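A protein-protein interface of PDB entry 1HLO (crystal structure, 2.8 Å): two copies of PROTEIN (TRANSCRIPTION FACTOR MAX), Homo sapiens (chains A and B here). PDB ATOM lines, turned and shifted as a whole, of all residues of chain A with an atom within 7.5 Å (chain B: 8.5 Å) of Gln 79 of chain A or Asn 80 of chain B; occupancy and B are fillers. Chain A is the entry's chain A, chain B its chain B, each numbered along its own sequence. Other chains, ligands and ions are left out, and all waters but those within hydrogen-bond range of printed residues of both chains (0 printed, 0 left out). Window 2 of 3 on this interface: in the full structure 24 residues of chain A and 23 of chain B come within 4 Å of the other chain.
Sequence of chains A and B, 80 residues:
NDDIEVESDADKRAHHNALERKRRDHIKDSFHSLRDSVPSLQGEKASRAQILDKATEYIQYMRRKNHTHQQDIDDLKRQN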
ATOM      1  N   ILE A  73       0.923  -0.674 -27.456  1.00  0.00           N
ATOM      2  CA  ILE A  73      -0.340  -0.191 -26.937  1.00  0.00           C
ATOM      3  C   ILE A  73      -1.403  -0.823 -27.839  1.00  0.00           C
ATOM      4  O   ILE A  73      -2.239  -1.582 -27.356  1.00  0.00           O
ATOM      5  CB  ILE A  73      -0.419   1.350 -26.950  1.00  0.00           C
ATOM      6  CG1 ILE A  73       0.500   1.917 -25.879  1.00  0.00           C
ATOM      7  CG2 ILE A  73      -1.851   1.821 -26.704  1.00  0.00           C
ATOM      8  CD1 ILE A  73       0.542   3.406 -25.859  1.00  0.00           C
ATOM      9  N   ASP A  74      -1.294  -0.610 -29.151  1.00  0.00           N
ATOM     10  CA  ASP A  74      -2.236  -1.171 -30.124  1.00  0.00           C
ATOM     11  C   ASP A  74      -2.435  -2.665 -29.931  1.00  0.00           C
ATOM     12  O   ASP A  74      -3.552  -3.162 -29.978  1.00  0.00           O
ATOM     13  CB  ASP A  74      -1.747  -0.940 -31.564  1.00  0.00           C
ATOM     14  CG  ASP A  74      -1.790   0.536 -31.986  1.00  0.00           C
ATOM     15  OD1 ASP A  74      -2.102   1.410 -31.140  1.00  0.00           O
ATOM     16  OD2 ASP A  74      -1.508   0.829 -33.174  1.00  0.00           O
ATOM     17  N   ASP A  75      -1.347  -3.377 -29.685  1.00  0.00           N
ATOM     18  CA  ASP A  75      -1.417  -4.815 -29.513  1.00  0.00           C
ATOM     19  C   ASP A  75      -1.930  -5.236 -28.154  1.00  0.00           C
ATOM     20  O   ASP A  75      -2.357  -6.370 -27.984  1.00  0.00           O
ATOM     21  CB  ASP A  75      -0.063  -5.452 -29.808  1.00  0.00           C
ATOM     22  CG  ASP A  75       0.611  -4.846 -31.035  1.00  0.00           C
ATOM     23  OD1 ASP A  75       1.856  -4.953 -31.134  1.00  0.00           O
ATOM     24  OD2 ASP A  75      -0.087  -4.242 -31.886  1.00  0.00           O
ATOM     25  N   LEU A  76      -1.885  -4.342 -27.179  1.00  0.00           N
ATOM     26  CA  LEU A  76      -2.396  -4.658 -25.854  1.00  0.00           C
ATOM     27  C   LEU A  76      -3.877  -4.255 -25.897  1.00  0.00           C
ATOM     28  O   LEU A  76      -4.703  -4.754 -25.141  1.00  0.00           O
ATOM     29  CB  LEU A  76      -1.603  -3.887 -24.788  1.00  0.00           C
ATOM     30  CG  LEU A  76      -1.555  -4.300 -23.308  1.00  0.00           C
ATOM     31  CD1 LEU A  76      -1.556  -5.803 -23.128  1.00  0.00           C
ATOM     32  CD2 LEU A  76      -0.323  -3.706 -22.649  1.00  0.00           C
ATOM     33  N   LYS A  77      -4.203  -3.402 -26.861  1.00  0.00           N
ATOM     34  CA  LYS A  77      -5.558  -2.920 -27.097  1.00  0.00           C
ATOM     35  C   LYS A  77      -6.287  -3.917 -28.004  1.00  0.00           C
ATOM     36  O   LYS A  77      -7.452  -3.726 -28.348  1.00  0.00           O
ATOM     37  CB  LYS A  77      -5.503  -1.556 -27.780  1.00  0.00           C
ATOM     38  CG  LYS A  77      -5.779  -0.375 -26.886  1.00  0.00           C
ATOM     39  CD  LYS A  77      -5.593   0.910 -27.687  1.00  0.00           C
ATOM     40  CE  LYS A  77      -5.924   2.144 -26.866  1.00  0.00           C
ATOM     41  NZ  LYS A  77      -7.387   2.249 -26.590  1.00  0.00           N
ATOM     42  N   ARG A  78      -5.560  -4.948 -28.428  1.00  0.00           N
ATOM     43  CA  ARG A  78      -6.086  -6.024 -29.270  1.00  0.00           C
ATOM     44  C   ARG A  78      -6.492  -7.090 -28.278  1.00  0.00           C
ATOM     45  O   ARG A  78      -7.538  -7.703 -28.392  1.00  0.00           O
ATOM     46  CB  ARG A  78      -4.973  -6.590 -30.155  1.00  0.00           C
ATOM     47  CG  ARG A  78      -5.330  -6.745 -31.614  1.00  0.00           C
ATOM     48  CD  ARG A  78      -5.689  -5.405 -32.220  1.00  0.00           C
ATOM     49  NE  ARG A  78      -7.117  -5.308 -32.495  1.00  0.00           N
ATOM     50  CZ  ARG A  78      -7.622  -4.673 -33.544  1.00  0.00           C
ATOM     51  NH1 ARG A  78      -6.808  -4.073 -34.405  1.00  0.00           N
ATOM     52  NH2 ARG A  78      -8.932  -4.674 -33.762  1.00  0.00           N
ATOM     53  N   GLN A  79      -5.575  -7.354 -27.358  1.00  0.00           N
ATOM     54  CA  GLN A  79      -5.760  -8.311 -26.287  1.00  0.00           C
ATOM     55  C   GLN A  79      -6.890  -7.845 -25.373  1.00  0.00           C
ATOM     56  O   GLN A  79      -7.645  -8.658 -24.839  1.00  0.00           O
ATOM     57  CB  GLN A  79      -4.466  -8.445 -25.488  1.00  0.00           C
ATOM     58  CG  GLN A  79      -3.416  -9.304 -26.162  1.00  0.00           C
ATOM     59  CD  GLN A  79      -2.314  -9.711 -25.201  1.00  0.00           C
ATOM     60  OE1 GLN A  79      -2.557  -9.887 -24.001  1.00  0.00           O
ATOM     61  NE2 GLN A  79      -1.094  -9.852 -25.717  1.00  0.00           N
ATOM     62  N   ASN A  80      -6.939  -6.545 -25.110  1.00  0.00           N
ATOM     63  CA  ASN A  80      -7.991  -5.990 -24.268  1.00  0.00           C
ATOM     64  C   ASN A  80      -9.247  -5.827 -25.119  1.00  0.00           C
ATOM     65  O   ASN A  80      -9.111  -5.797 -26.366  1.00  0.00           O
ATOM     66  CB  ASN A  80      -7.561  -4.637 -23.685  1.00  0.00           C
ATOM     67  CG  ASN A  80      -8.679  -3.945 -22.913  1.00  0.00           C
ATOM     68  OD1 ASN A  80      -9.131  -2.844 -23.266  1.00  0.00           O
ATOM     69  ND2 ASN A  80      -9.116  -4.581 -21.837  1.00  0.00           N
ATOM     70  N   ILE B  73       0.776   1.477 -20.689  1.00  0.00           N
ATOM     71  CA  ILE B  73       1.182   0.119 -21.003  1.00  0.00           C
ATOM     72  C   ILE B  73       0.994  -0.655 -19.698  1.00  0.00           C
ATOM     73  O   ILE B  73       0.208  -1.585 -19.657  1.00  0.00           O
ATOM     74  CB  ILE B  73       2.620   0.086 -21.533  1.00  0.00           C
ATOM     75  CG1 ILE B  73       2.607   0.363 -23.043  1.00  0.00           C
ATOM     76  CG2 ILE B  73       3.292  -1.204 -21.186  1.00  0.00           C
ATOM     77  CD1 ILE B  73       3.987   0.690 -23.646  1.00  0.00           C
ATOM     78  N   ASP B  74       1.608  -0.190 -18.611  1.00  0.00           N
ATOM     79  CA  ASP B  74       1.462  -0.830 -17.305  1.00  0.00           C
ATOM     80  C   ASP B  74       0.008  -1.068 -16.928  1.00  0.00           C
ATOM     81  O   ASP B  74      -0.348  -2.116 -16.408  1.00  0.00           O
ATOM     82  CB  ASP B  74       2.066   0.030 -16.194  1.00  0.00           C
ATOM     83  CG  ASP B  74       3.565   0.190 -16.316  1.00  0.00           C
ATOM     84  OD1 ASP B  74       4.161  -0.443 -17.228  1.00  0.00           O
ATOM     85  OD2 ASP B  74       4.139   0.946 -15.481  1.00  0.00           O
ATOM     86  N   ASP B  75      -0.837  -0.088 -17.177  1.00  0.00           N
ATOM     87  CA  ASP B  75      -2.236  -0.224 -16.831  1.00  0.00           C
ATOM     88  C   ASP B  75      -3.024  -1.088 -17.785  1.00  0.00           C
ATOM     89  O   ASP B  75      -4.093  -1.562 -17.447  1.00  0.00           O
ATOM     90  CB  ASP B  75      -2.872   1.147 -16.638  1.00  0.00           C
ATOM     91  CG  ASP B  75      -2.329   1.860 -15.408  1.00  0.00           C
ATOM     92  OD1 ASP B  75      -1.564   1.236 -14.632  1.00  0.00           O
ATOM     93  OD2 ASP B  75      -2.656   3.048 -15.219  1.00  0.00           O
ATOM     94  N   LEU B  76      -2.513  -1.293 -18.985  1.00  0.00           N
ATOM     95  CA  LEU B  76      -3.208  -2.150 -19.927  1.00  0.00           C
ATOM     96  C   LEU B  76      -2.685  -3.553 -19.655  1.00  0.00           C
ATOM     97  O   LEU B  76      -3.314  -4.542 -20.010  1.00  0.00           O
ATOM     98  CB  LEU B  76      -2.918  -1.718 -21.367  1.00  0.00           C
ATOM     99  CG  LEU B  76      -4.203  -1.499 -22.154  1.00  0.00           C
ATOM    100  CD1 LEU B  76      -5.090  -0.593 -21.336  1.00  0.00           C
ATOM    101  CD2 LEU B  76      -3.925  -0.906 -23.533  1.00  0.00           C
ATOM    102  N   LYS B  77      -1.542  -3.603 -18.974  1.00  0.00           N
ATOM    103  CA  LYS B  77      -0.851  -4.826 -18.579  1.00  0.00           C
ATOM    104  C   LYS B  77      -1.355  -5.246 -17.194  1.00  0.00           C
ATOM    105  O   LYS B  77      -1.082  -6.346 -16.722  1.00  0.00           O
ATOM    106  CB  LYS B  77       0.649  -4.522 -18.543  1.00  0.00           C
ATOM    107  CG  LYS B  77       1.572  -5.545 -17.939  1.00  0.00           C
ATOM    108  CD  LYS B  77       3.020  -5.146 -18.215  1.00  0.00           C
ATOM    109  CE  LYS B  77       3.307  -5.072 -19.716  1.00  0.00           C
ATOM    110  NZ  LYS B  77       4.746  -4.738 -19.982  1.00  0.00           N
ATOM    111  N   ARG B  78      -1.910  -4.280 -16.473  1.00  0.00           N
ATOM    112  CA  ARG B  78      -2.485  -4.538 -15.163  1.00  0.00           C
ATOM    113  C   ARG B  78      -3.957  -4.775 -15.410  1.00  0.00           C
ATOM    114  O   ARG B  78      -4.673  -5.256 -14.545  1.00  0.00           O
ATOM    115  CB  ARG B  78      -2.310  -3.332 -14.240  1.00  0.00           C
ATOM    116  CG  ARG B  78      -1.100  -3.449 -13.364  1.00  0.00           C
ATOM    117  CD  ARG B  78      -0.280  -2.175 -13.329  1.00  0.00           C
ATOM    118  NE  ARG B  78       1.137  -2.511 -13.181  1.00  0.00           N
ATOM    119  CZ  ARG B  78       1.994  -1.887 -12.374  1.00  0.00           C
ATOM    120  NH1 ARG B  78       1.593  -0.869 -11.618  1.00  0.00           N
ATOM    121  NH2 ARG B  78       3.257  -2.300 -12.307  1.00  0.00           N
ATOM    122  N   GLN B  79      -4.410  -4.402 -16.599  1.00  0.00           N
ATOM    123  CA  GLN B  79      -5.807  -4.567 -16.944  1.00  0.00           C
ATOM    124  C   GLN B  79      -6.007  -5.909 -17.624  1.00  0.00           C
ATOM    125  O   GLN B  79      -6.996  -6.595 -17.360  1.00  0.00           O
ATOM    126  CB  GLN B  79      -6.251  -3.433 -17.859  1.00  0.00           C
ATOM    127  CG  GLN B  79      -7.727  -3.355 -18.118  1.00  0.00           C
ATOM    128  CD  GLN B  79      -8.059  -2.339 -19.192  1.00  0.00           C
ATOM    129  OE1 GLN B  79      -8.662  -1.296 -18.925  1.00  0.00           O
ATOM    130  NE2 GLN B  79      -7.668  -2.643 -20.421  1.00  0.00           N
ATOM    131  N   ASN B  80      -5.099  -6.261 -18.531  1.00  0.00           N
ATOM    132  CA  ASN B  80      -5.182  -7.538 -19.234  1.00  0.00           C
ATOM    133  C   ASN B  80      -4.549  -8.653 -18.415  1.00  0.00           C
ATOM    134  O   ASN B  80      -3.800  -8.324 -17.467  1.00  0.00           O
ATOM    135  CB  ASN B  80      -4.533  -7.447 -20.614  1.00  0.00           C
ATOM    136  CG  ASN B  80      -5.535  -7.092 -21.679  1.00  0.00           C
ATOM    137  OD1 ASN B  80      -6.334  -6.161 -21.525  1.00  0.00           O
ATOM    138  ND2 ASN B  80      -5.542  -7.856 -22.745  1.00  0.00           N
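O of Gln 79 of chain A lies close to ND2 of Asn 80 of chain B (3.1 Å).
ND2 of Asn 80 of chain A sits close to NE2 of Gln 79 of chain B, at 2.8 Å.
The backbone NH (N) of Asn 80 of chain A sits close to the side-chain amide nitrogen (ND2) of Asn 80 of chain B (3.0 Å).
Ile 73 of chain B touches Ile 73 of chain A.
Leu 76 of chain A touches Ile 73 of chain B.
Leu 76 of chain B touches Leu 76 of chain A.
Leu 76 of chain A touches Lys 77 of chain B.
Lys 77 of chain A touches Leu 76 of chain B (CG to CD2, 3.9 Å).
Asp 75 of chain A touches none of the printed residues of chain B.
Of the printed residues of chain B, Leu 76 of chain A touches Ile 73 (3.7 Å), Leu 76 (3.5 Å) and Lys 77 (3.9 Å).
Gln 79 of chain A touches just one residue of chain B: Asn 80.
Of the printed residues of chain B, Asn 80 of chain A touches Gln 79 (2.8 Å) and Asn 80 (2.9 Å).
Asp 75 of chain B touches none of the printed residues of chain A.
Of the printed residues of chain A, Gln 79 of chain B touches Asn 80 (2.8 Å).
Printed residues of chain A within 4 Å of Asn 80 of chain B: Gln 79 (3.0 Å) and Asn 80 (2.9 Å).
The nearest residue of chain B that does not touch Gln 79 of chain A is Leu 76 of chain B (6.7 Å).
The nearest printed residue of chain A that does not touch Gln 79 of chain B is Leu 76 of chain A (6.0 Å).
Of the 8 printed residues of chain A, 5 touch a printed residue of chain B.
Hydrophobic or aromatic side chains of chain A that line the printed part of chain B: Ile 73 and Leu 76.
Among the printed residues, no Asp or Glu carboxylate lies within 4 Å of a Lys or Arg side-chain nitrogen of the other chain.
Ile 73 of chain A touches its own counterpart, Ile 73 of chain B.
Leu 76 of chain A touches Ile 73 of chain B, but with the chains exchanged Ile 73 of chain A does not touch Leu 76 of chain B (4.2 Å).
Leu 76 of chain A touches its own counterpart, Leu 76 of chain B.
Asn 80 of chain A touches its own counterpart, Asn 80 of chain B.
8 positions are printed for both chains.
Of the 8 pairs that touch across the chains among the printed residues, 7 have their exchanged pair printed and touching as well.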
